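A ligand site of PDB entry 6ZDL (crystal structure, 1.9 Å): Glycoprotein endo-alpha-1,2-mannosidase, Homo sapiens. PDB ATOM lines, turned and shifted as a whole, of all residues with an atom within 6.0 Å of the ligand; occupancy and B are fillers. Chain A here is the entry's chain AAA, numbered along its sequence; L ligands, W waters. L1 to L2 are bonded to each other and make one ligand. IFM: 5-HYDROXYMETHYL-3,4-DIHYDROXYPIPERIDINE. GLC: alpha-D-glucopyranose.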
ATOM      1  N   TYR A  28     -16.285 -17.134  -2.699  1.00  0.00           N
ATOM      2  CA  TYR A  28     -17.679 -16.746  -2.758  1.00  0.00           C
ATOM      3  C   TYR A  28     -18.545 -17.966  -2.405  1.00  0.00           C
ATOM      4  O   TYR A  28     -18.318 -19.052  -2.938  1.00  0.00           O
ATOM      5  CB  TYR A  28     -17.975 -16.166  -4.138  1.00  0.00           C
ATOM      6  CG  TYR A  28     -17.171 -14.905  -4.333  1.00  0.00           C
ATOM      7  CD1 TYR A  28     -15.845 -14.969  -4.758  1.00  0.00           C
ATOM      8  CD2 TYR A  28     -17.685 -13.659  -3.977  1.00  0.00           C
ATOM      9  CE1 TYR A  28     -15.075 -13.825  -4.884  1.00  0.00           C
ATOM     10  CE2 TYR A  28     -16.922 -12.511  -4.109  1.00  0.00           C
ATOM     11  CZ  TYR A  28     -15.607 -12.601  -4.537  1.00  0.00           C
ATOM     12  OH  TYR A  28     -14.820 -11.480  -4.665  1.00  0.00           O
ATOM     13  N   TRP A  30     -22.120 -17.750  -2.493  1.00  0.00           N
ATOM     14  CA  TRP A  30     -23.463 -17.279  -2.855  1.00  0.00           C
ATOM     15  C   TRP A  30     -24.184 -18.080  -3.971  1.00  0.00           C
ATOM     16  O   TRP A  30     -25.240 -17.645  -4.440  1.00  0.00           O
ATOM     17  CB  TRP A  30     -23.395 -15.794  -3.229  1.00  0.00           C
ATOM     18  CG  TRP A  30     -22.446 -15.432  -4.390  1.00  0.00           C
ATOM     19  CD1 TRP A  30     -21.978 -16.266  -5.406  1.00  0.00           C
ATOM     20  CD2 TRP A  30     -21.905 -14.131  -4.680  1.00  0.00           C
ATOM     21  NE1 TRP A  30     -21.172 -15.542  -6.273  1.00  0.00           N
ATOM     22  CE2 TRP A  30     -21.117 -14.240  -5.864  1.00  0.00           C
ATOM     23  CE3 TRP A  30     -22.014 -12.883  -4.051  1.00  0.00           C
ATOM     24  CZ2 TRP A  30     -20.431 -13.159  -6.412  1.00  0.00           C
ATOM     25  CZ3 TRP A  30     -21.328 -11.802  -4.599  1.00  0.00           C
ATOM     26  CH2 TRP A  30     -20.535 -11.961  -5.770  1.00  0.00           C
ATOM     27  N   HIS A  42     -27.571 -16.996  -8.149  1.00  0.00           N
ATOM     28  CA  HIS A  42     -26.383 -16.502  -8.863  1.00  0.00           C
ATOM     29  C   HIS A  42     -26.105 -17.119 -10.244  1.00  0.00           C
ATOM     30  O   HIS A  42     -25.802 -16.387 -11.167  1.00  0.00           O
ATOM     31  CB  HIS A  42     -25.113 -16.505  -7.961  1.00  0.00           C
ATOM     32  CG  HIS A  42     -24.990 -15.265  -7.126  1.00  0.00           C
ATOM     33  ND1 HIS A  42     -24.177 -14.199  -7.478  1.00  0.00           N
ATOM     34  CD2 HIS A  42     -25.570 -14.905  -5.950  1.00  0.00           C
ATOM     35  CE1 HIS A  42     -24.288 -13.253  -6.576  1.00  0.00           C
ATOM     36  NE2 HIS A  42     -25.134 -13.656  -5.640  1.00  0.00           N
ATOM     37  N   HIS A  45     -28.049 -15.369 -12.828  1.00  0.00           N
ATOM     38  CA  HIS A  45     -27.790 -13.935 -12.659  1.00  0.00           C
ATOM     39  C   HIS A  45     -28.490 -13.135 -13.752  1.00  0.00           C
ATOM     40  O   HIS A  45     -28.571 -13.583 -14.901  1.00  0.00           O
ATOM     41  CB  HIS A  45     -26.280 -13.649 -12.701  1.00  0.00           C
ATOM     42  CG  HIS A  45     -25.873 -12.402 -11.991  1.00  0.00           C
ATOM     43  ND1 HIS A  45     -26.121 -11.144 -12.499  1.00  0.00           N
ATOM     44  CD2 HIS A  45     -25.171 -12.217 -10.841  1.00  0.00           C
ATOM     45  CE1 HIS A  45     -25.625 -10.236 -11.673  1.00  0.00           C
ATOM     46  NE2 HIS A  45     -25.047 -10.858 -10.656  1.00  0.00           N
ATOM     47  N   LEU A  48     -27.046  -7.196 -16.162  1.00  0.00           N
ATOM     48  CA  LEU A  48     -27.076  -5.900 -15.514  1.00  0.00           C
ATOM     49  C   LEU A  48     -27.232  -4.814 -16.562  1.00  0.00           C
ATOM     50  O   LEU A  48     -26.473  -4.773 -17.524  1.00  0.00           O
ATOM     51  CB  LEU A  48     -25.807  -5.672 -14.666  1.00  0.00           C
ATOM     52  CG  LEU A  48     -25.616  -6.668 -13.514  1.00  0.00           C
ATOM     53  CD1 LEU A  48     -24.378  -6.346 -12.688  1.00  0.00           C
ATOM     54  CD2 LEU A  48     -26.835  -6.783 -12.597  1.00  0.00           C
ATOM     55  N   SER A 107     -16.184 -13.907   1.091  1.00  0.00           N
ATOM     56  CA  SER A 107     -17.140 -12.821   0.855  1.00  0.00           C
ATOM     57  C   SER A 107     -18.267 -12.927   1.888  1.00  0.00           C
ATOM     58  O   SER A 107     -18.849 -13.997   2.070  1.00  0.00           O
ATOM     59  CB  SER A 107     -17.702 -12.903  -0.576  1.00  0.00           C
ATOM     60  OG  SER A 107     -18.761 -11.991  -0.797  1.00  0.00           O
ATOM     61  N   TYR A 109     -21.614 -10.970   4.051  1.00  0.00           N
ATOM     62  CA  TYR A 109     -22.645 -10.012   4.415  1.00  0.00           C
ATOM     63  C   TYR A 109     -23.159 -10.366   5.834  1.00  0.00           C
ATOM     64  O   TYR A 109     -23.130 -11.525   6.232  1.00  0.00           O
ATOM     65  CB  TYR A 109     -23.812 -10.058   3.420  1.00  0.00           C
ATOM     66  CG  TYR A 109     -23.555  -9.303   2.121  1.00  0.00           C
ATOM     67  CD1 TYR A 109     -22.889  -9.905   1.043  1.00  0.00           C
ATOM     68  CD2 TYR A 109     -23.937  -7.983   1.996  1.00  0.00           C
ATOM     69  CE1 TYR A 109     -22.661  -9.205  -0.136  1.00  0.00           C
ATOM     70  CE2 TYR A 109     -23.717  -7.279   0.812  1.00  0.00           C
ATOM     71  CZ  TYR A 109     -23.078  -7.903  -0.246  1.00  0.00           C
ATOM     72  OH  TYR A 109     -22.840  -7.180  -1.387  1.00  0.00           O
ATOM     73  N   ASP A 115     -26.010  -9.866  -0.876  1.00  0.00           N
ATOM     74  CA  ASP A 115     -25.762  -9.129  -2.108  1.00  0.00           C
ATOM     75  C   ASP A 115     -27.090  -9.011  -2.845  1.00  0.00           C
ATOM     76  O   ASP A 115     -28.024  -9.805  -2.647  1.00  0.00           O
ATOM     77  CB  ASP A 115     -24.667  -9.789  -2.964  1.00  0.00           C
ATOM     78  CG  ASP A 115     -25.217 -10.862  -3.902  1.00  0.00           C
ATOM     79  OD1 ASP A 115     -25.368 -12.024  -3.472  1.00  0.00           O
ATOM     80  OD2 ASP A 115     -25.468 -10.534  -5.089  1.00  0.00           O
ATOM     81  N   GLU A 116     -27.155  -8.010  -3.700  1.00  0.00           N
ATOM     82  CA  GLU A 116     -28.387  -7.664  -4.424  1.00  0.00           C
ATOM     83  C   GLU A 116     -28.876  -8.762  -5.384  1.00  0.00           C
ATOM     84  O   GLU A 116     -30.044  -8.787  -5.738  1.00  0.00           O
ATOM     85  CB  GLU A 116     -28.198  -6.323  -5.149  1.00  0.00           C
ATOM     86  CG  GLU A 116     -26.982  -6.236  -6.080  1.00  0.00           C
ATOM     87  CD  GLU A 116     -25.675  -5.756  -5.410  1.00  0.00           C
ATOM     88  OE1 GLU A 116     -25.344  -6.207  -4.266  1.00  0.00           O
ATOM     89  OE2 GLU A 116     -24.953  -4.952  -6.046  1.00  0.00           O
ATOM     90  N   ASN A 117     -28.003  -9.703  -5.765  1.00  0.00           N
ATOM     91  CA  ASN A 117     -28.374 -10.807  -6.651  1.00  0.00           C
ATOM     92  C   ASN A 117     -28.412 -12.156  -5.949  1.00  0.00           C
ATOM     93  O   ASN A 117     -28.505 -13.172  -6.623  1.00  0.00           O
ATOM     94  CB  ASN A 117     -27.414 -10.856  -7.856  1.00  0.00           C
ATOM     95  CG  ASN A 117     -27.480  -9.593  -8.692  1.00  0.00           C
ATOM     96  OD1 ASN A 117     -26.571  -8.753  -8.655  1.00  0.00           O
ATOM     97  ND2 ASN A 117     -28.580  -9.422  -9.403  1.00  0.00           N
ATOM     98  N   GLY A 118     -28.375 -12.168  -4.614  1.00  0.00           N
ATOM     99  CA  GLY A 118     -28.271 -13.416  -3.850  1.00  0.00           C
ATOM    100  C   GLY A 118     -29.191 -13.538  -2.653  1.00  0.00           C
ATOM    101  O   GLY A 118     -30.122 -12.740  -2.485  1.00  0.00           O
ATOM    102  N   HIS A 142     -14.041 -11.126   3.981  1.00  0.00           N
ATOM    103  CA  HIS A 142     -14.042 -10.101   2.939  1.00  0.00           C
ATOM    104  C   HIS A 142     -15.376  -9.372   3.066  1.00  0.00           C
ATOM    105  O   HIS A 142     -16.381  -9.812   2.529  1.00  0.00           O
ATOM    106  CB  HIS A 142     -13.867 -10.742   1.552  1.00  0.00           C
ATOM    107  CG  HIS A 142     -13.618  -9.755   0.431  1.00  0.00           C
ATOM    108  ND1 HIS A 142     -13.713 -10.114  -0.902  1.00  0.00           N
ATOM    109  CD2 HIS A 142     -13.258  -8.448   0.441  1.00  0.00           C
ATOM    110  CE1 HIS A 142     -13.441  -9.054  -1.655  1.00  0.00           C
ATOM    111  NE2 HIS A 142     -13.147  -8.038  -0.868  1.00  0.00           N
ATOM    112  N   GLU A 144     -18.353  -7.151   2.560  1.00  0.00           N
ATOM    113  CA  GLU A 144     -18.931  -6.563   1.365  1.00  0.00           C
ATOM    114  C   GLU A 144     -19.631  -5.253   1.736  1.00  0.00           C
ATOM    115  O   GLU A 144     -19.860  -4.986   2.930  1.00  0.00           O
ATOM    116  CB  GLU A 144     -19.858  -7.589   0.706  1.00  0.00           C
ATOM    117  CG  GLU A 144     -19.135  -8.847   0.202  1.00  0.00           C
ATOM    118  CD  GLU A 144     -18.434  -8.667  -1.150  1.00  0.00           C
ATOM    119  OE1 GLU A 144     -18.464  -7.562  -1.686  1.00  0.00           O
ATOM    120  OE2 GLU A 144     -17.868  -9.650  -1.694  1.00  0.00           O
ATOM    121  N   PRO A 145     -19.941  -4.416   0.733  1.00  0.00           N
ATOM    122  CA  PRO A 145     -20.556  -3.118   1.009  1.00  0.00           C
ATOM    123  C   PRO A 145     -22.067  -3.242   1.140  1.00  0.00           C
ATOM    124  O   PRO A 145     -22.785  -2.986   0.199  1.00  0.00           O
ATOM    125  CB  PRO A 145     -20.151  -2.266  -0.206  1.00  0.00           C
ATOM    126  CG  PRO A 145     -19.981  -3.263  -1.302  1.00  0.00           C
ATOM    127  CD  PRO A 145     -19.491  -4.517  -0.661  1.00  0.00           C
ATOM    128  N   TYR A 188     -14.164  -4.390   1.235  1.00  0.00           N
ATOM    129  CA  TYR A 188     -14.434  -4.037  -0.171  1.00  0.00           C
ATOM    130  C   TYR A 188     -15.188  -2.712  -0.277  1.00  0.00           C
ATOM    131  O   TYR A 188     -16.151  -2.475   0.447  1.00  0.00           O
ATOM    132  CB  TYR A 188     -15.221  -5.121  -0.922  1.00  0.00           C
ATOM    133  CG  TYR A 188     -15.316  -4.827  -2.413  1.00  0.00           C
ATOM    134  CD1 TYR A 188     -14.215  -5.023  -3.266  1.00  0.00           C
ATOM    135  CD2 TYR A 188     -16.494  -4.334  -2.987  1.00  0.00           C
ATOM    136  CE1 TYR A 188     -14.290  -4.722  -4.623  1.00  0.00           C
ATOM    137  CE2 TYR A 188     -16.584  -4.027  -4.338  1.00  0.00           C
ATOM    138  CZ  TYR A 188     -15.485  -4.227  -5.156  1.00  0.00           C
ATOM    139  OH  TYR A 188     -15.588  -3.930  -6.497  1.00  0.00           O
ATOM    140  N   TYR A 241      -5.277  -3.429  -0.269  1.00  0.00           N
ATOM    141  CA  TYR A 241      -5.381  -4.420  -1.330  1.00  0.00           C
ATOM    142  C   TYR A 241      -6.050  -3.776  -2.529  1.00  0.00           C
ATOM    143  O   TYR A 241      -6.680  -2.717  -2.410  1.00  0.00           O
ATOM    144  CB  TYR A 241      -6.064  -5.731  -0.885  1.00  0.00           C
ATOM    145  CG  TYR A 241      -7.588  -5.711  -0.815  1.00  0.00           C
ATOM    146  CD1 TYR A 241      -8.264  -4.847   0.049  1.00  0.00           C
ATOM    147  CD2 TYR A 241      -8.352  -6.612  -1.560  1.00  0.00           C
ATOM    148  CE1 TYR A 241      -9.643  -4.862   0.139  1.00  0.00           C
ATOM    149  CE2 TYR A 241      -9.738  -6.624  -1.476  1.00  0.00           C
ATOM    150  CZ  TYR A 241     -10.372  -5.753  -0.626  1.00  0.00           C
ATOM    151  OH  TYR A 241     -11.758  -5.766  -0.525  1.00  0.00           O
ATOM    152  N   TYR A 243      -7.686  -5.727  -5.319  1.00  0.00           N
ATOM    153  CA  TYR A 243      -8.745  -6.596  -5.830  1.00  0.00           C
ATOM    154  C   TYR A 243      -8.806  -6.910  -7.348  1.00  0.00           C
ATOM    155  O   TYR A 243      -8.694  -8.065  -7.713  1.00  0.00           O
ATOM    156  CB  TYR A 243     -10.117  -6.238  -5.293  1.00  0.00           C
ATOM    157  CG  TYR A 243     -11.082  -7.330  -5.634  1.00  0.00           C
ATOM    158  CD1 TYR A 243     -11.216  -8.451  -4.799  1.00  0.00           C
ATOM    159  CD2 TYR A 243     -11.805  -7.291  -6.834  1.00  0.00           C
ATOM    160  CE1 TYR A 243     -12.072  -9.497  -5.143  1.00  0.00           C
ATOM    161  CE2 TYR A 243     -12.646  -8.334  -7.195  1.00  0.00           C
ATOM    162  CZ  TYR A 243     -12.783  -9.431  -6.358  1.00  0.00           C
ATOM    163  OH  TYR A 243     -13.619 -10.432  -6.766  1.00  0.00           O
ATOM    164  N   ASP A 282     -16.574 -10.428 -17.823  1.00  0.00           N
ATOM    165  CA  ASP A 282     -17.871 -10.375 -17.132  1.00  0.00           C
ATOM    166  C   ASP A 282     -19.026 -10.098 -18.084  1.00  0.00           C
ATOM    167  O   ASP A 282     -20.138  -9.788 -17.645  1.00  0.00           O
ATOM    168  CB  ASP A 282     -17.848  -9.345 -15.977  1.00  0.00           C
ATOM    169  CG  ASP A 282     -17.760  -7.919 -16.449  1.00  0.00           C
ATOM    170  OD1 ASP A 282     -17.716  -7.651 -17.682  1.00  0.00           O
ATOM    171  OD2 ASP A 282     -17.699  -7.028 -15.574  1.00  0.00           O
ATOM    172  N   ILE A 285     -22.876 -10.953 -17.855  1.00  0.00           N
ATOM    173  CA  ILE A 285     -23.715 -10.113 -16.977  1.00  0.00           C
ATOM    174  C   ILE A 285     -23.495  -8.617 -17.134  1.00  0.00           C
ATOM    175  O   ILE A 285     -24.386  -7.838 -16.752  1.00  0.00           O
ATOM    176  CB  ILE A 285     -23.616 -10.502 -15.483  1.00  0.00           C
ATOM    177  CG1 ILE A 285     -22.202 -10.279 -14.942  1.00  0.00           C
ATOM    178  CG2 ILE A 285     -24.059 -11.946 -15.271  1.00  0.00           C
ATOM    179  CD1 ILE A 285     -22.157  -9.930 -13.468  1.00  0.00           C
ATOM    180  N   ARG A 286     -22.352  -8.185 -17.677  1.00  0.00           N
ATOM    181  CA  ARG A 286     -22.092  -6.781 -17.999  1.00  0.00           C
ATOM    182  C   ARG A 286     -21.623  -6.705 -19.457  1.00  0.00           C
ATOM    183  O   ARG A 286     -20.460  -6.459 -19.732  1.00  0.00           O
ATOM    184  CB  ARG A 286     -21.065  -6.165 -17.043  1.00  0.00           C
ATOM    185  CG  ARG A 286     -21.397  -6.326 -15.569  1.00  0.00           C
ATOM    186  CD  ARG A 286     -20.596  -5.372 -14.679  1.00  0.00           C
ATOM    187  NE  ARG A 286     -20.770  -5.703 -13.272  1.00  0.00           N
ATOM    188  CZ  ARG A 286     -20.049  -6.579 -12.551  1.00  0.00           C
ATOM    189  NH1 ARG A 286     -19.018  -7.262 -13.081  1.00  0.00           N
ATOM    190  NH2 ARG A 286     -20.360  -6.774 -11.265  1.00  0.00           N
ATOM    191  N   GLU A 324     -15.239 -16.358  -8.397  1.00  0.00           N
ATOM    192  CA  GLU A 324     -16.118 -15.304  -8.922  1.00  0.00           C
ATOM    193  C   GLU A 324     -16.344 -15.626 -10.413  1.00  0.00           C
ATOM    194  O   GLU A 324     -15.616 -15.145 -11.306  1.00  0.00           O
ATOM    195  CB  GLU A 324     -15.555 -13.895  -8.667  1.00  0.00           C
ATOM    196  CG  GLU A 324     -16.606 -12.850  -8.237  1.00  0.00           C
ATOM    197  CD  GLU A 324     -17.703 -12.543  -9.277  1.00  0.00           C
ATOM    198  OE1 GLU A 324     -18.470 -11.574  -9.063  1.00  0.00           O
ATOM    199  OE2 GLU A 324     -17.841 -13.244 -10.295  1.00  0.00           O
ATOM    200  N   HIS A 326     -18.956 -15.028 -12.380  1.00  0.00           N
ATOM    201  CA  HIS A 326     -19.534 -13.926 -13.183  1.00  0.00           C
ATOM    202  C   HIS A 326     -18.472 -13.087 -13.860  1.00  0.00           C
ATOM    203  O   HIS A 326     -18.673 -12.655 -14.989  1.00  0.00           O
ATOM    204  CB  HIS A 326     -20.421 -13.004 -12.363  1.00  0.00           C
ATOM    205  CG  HIS A 326     -21.379 -13.726 -11.480  1.00  0.00           C
ATOM    206  ND1 HIS A 326     -22.228 -14.696 -11.974  1.00  0.00           N
ATOM    207  CD2 HIS A 326     -21.568 -13.693 -10.144  1.00  0.00           C
ATOM    208  CE1 HIS A 326     -22.940 -15.182 -10.965  1.00  0.00           C
ATOM    209  NE2 HIS A 326     -22.551 -14.609  -9.843  1.00  0.00           N
ATOM    210  N   GLU A 327     -17.361 -12.842 -13.168  1.00  0.00           N
ATOM    211  CA  GLU A 327     -16.309 -11.943 -13.653  1.00  0.00           C
ATOM    212  C   GLU A 327     -15.169 -12.642 -14.331  1.00  0.00           C
ATOM    213  O   GLU A 327     -14.205 -12.006 -14.758  1.00  0.00           O
ATOM    214  CB  GLU A 327     -15.821 -11.062 -12.487  1.00  0.00           C
ATOM    215  CG  GLU A 327     -16.952 -10.139 -12.037  1.00  0.00           C
ATOM    216  CD  GLU A 327     -16.657  -9.180 -10.890  1.00  0.00           C
ATOM    217  OE1 GLU A 327     -15.804  -9.455 -10.025  1.00  0.00           O
ATOM    218  OE2 GLU A 327     -17.338  -8.135 -10.856  1.00  0.00           O
HETATM  219  O4  IFM L   1     -18.873  -7.021  -4.219  1.00  0.00           O
HETATM  220  C4  IFM L   1     -18.320  -7.967  -5.119  1.00  0.00           C
HETATM  221  C3  IFM L   1     -19.020  -7.741  -6.486  1.00  0.00           C
HETATM  222  O3  IFM L   1     -20.413  -8.035  -6.336  1.00  0.00           O
HETATM  223  C2  IFM L   1     -18.403  -8.599  -7.585  1.00  0.00           C
HETATM  224  N   IFM L   1     -16.971  -8.420  -7.547  1.00  0.00           N
HETATM  225  C1  IFM L   1     -16.272  -8.700  -6.318  1.00  0.00           C
HETATM  226  C5  IFM L   1     -16.802  -7.784  -5.239  1.00  0.00           C
HETATM  227  C6  IFM L   1     -16.026  -8.020  -3.939  1.00  0.00           C
HETATM  228  O6  IFM L   1     -16.198  -9.351  -3.439  1.00  0.00           O
HETATM  229  C1  GLC L   2     -21.217  -7.380  -7.325  1.00  0.00           C
HETATM  230  C2  GLC L   2     -22.641  -7.376  -6.818  1.00  0.00           C
HETATM  231  C3  GLC L   2     -23.226  -8.771  -6.829  1.00  0.00           C
HETATM  232  C4  GLC L   2     -23.106  -9.362  -8.237  1.00  0.00           C
HETATM  233  C5  GLC L   2     -21.644  -9.370  -8.657  1.00  0.00           C
HETATM  234  C6  GLC L   2     -21.495  -9.895 -10.075  1.00  0.00           C
HETATM  235  O2  GLC L   2     -22.636  -6.836  -5.496  1.00  0.00           O
HETATM  236  O3  GLC L   2     -24.601  -8.684  -6.486  1.00  0.00           O
HETATM  237  O4  GLC L   2     -23.644 -10.679  -8.239  1.00  0.00           O
HETATM  238  O5  GLC L   2     -21.184  -8.009  -8.614  1.00  0.00           O
HETATM  239  O6  GLC L   2     -20.120  -9.819 -10.484  1.00  0.00           O
HETATM  240  O   HOH W   1     -21.432  -8.251  -3.377  1.00  0.00           O
HETATM  241  O   HOH W   2     -20.459  -5.146  -4.825  1.00  0.00           O
HETATM  242  O   HOH W   3     -15.959  -5.731  -8.208  1.00  0.00           O
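Residues that only touch the ligand: His 42 (3.1 Å), Tyr 243 (3.2 Å), His 142 (3.3 Å), Ile 285 (3.5 Å), Tyr 188 (3.6 Å), His 326 (3.7 Å) and Trp 30 (3.97 Å).
Hydrophobic or aromatic side chains within 4 Å of the ligand: Tyr 28, Trp 30, His 42, His 45, His 142, Tyr 188, Tyr 243, Ile 285 and His 326.
The side-chain hydroxyl (OH) of Tyr 241 lies close to the backbone NH (N) of Tyr 188 (3.3 Å).
A ring nitrogen (NE2) of His 142 sits at hydrogen-bond distance from the side-chain hydroxyl (OH) of Tyr 241 (2.7 Å).
The backbone NH (N) of Gly 118 sits at hydrogen-bond distance from the side-chain carboxylate (OD1) of Asp 115.
The side-chain carboxylate (OD1) of Asp 115 lies within hydrogen-bond range of a ring nitrogen (NE2) of His 42 (2.7 Å).
OD2 of Asp 282 lies within salt-bridge range of NH1 of Arg 286 (2.8 Å).
The backbone NH (N) of Glu 327 is in hydrogen-bond range of the side-chain carboxylate (OE2) of Glu 324 (2.9 Å).
N of Leu 48 sits at hydrogen-bond distance from O of Ile 285.
OH of Tyr 243 lies within hydrogen-bond range of OH of Tyr 28 (2.6 Å).
O4 of GLC L2 is in hydrogen-bond range of NE2 of His 45, 2.8 Å away.
The side-chain carboxylate (OE2) of Glu 116 sits at hydrogen-bond distance from an oxygen (O2) of GLC L2, at 3.0 Å.
The guanidinium group of Arg 286 is in hydrogen-bond range of an oxygen (O5) of GLC L2 (3.0 Å).
O6 of IFM L1 is in hydrogen-bond range of OH of Tyr 28 (2.8 Å).
The side-chain carboxylate of Glu 327 lies within salt-bridge range of a nitrogen (N) of IFM L1, at 2.9 Å.
O6 of IFM L1 sits at hydrogen-bond distance from OE2 of Glu 144, at 2.4 Å.
OD1 of Asn 117 sits at hydrogen-bond distance from O3 of GLC L2, 2.9 Å away.
The side-chain carboxylate of Glu 324 is in salt-bridge range of a nitrogen (N) of IFM L1, at 3.8 Å.
O3 of GLC L2 lies within hydrogen-bond range of OD2 of Asp 115, 2.5 Å away.
Water W1 lies within hydrogen-bond range of the side-chain hydroxyl of Tyr 109, an oxygen (O2) of GLC L2 and the side-chain carboxylate of Glu 144.
Water W3 lies within hydrogen-bond range of OH of Tyr 188 and N of IFM L1.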
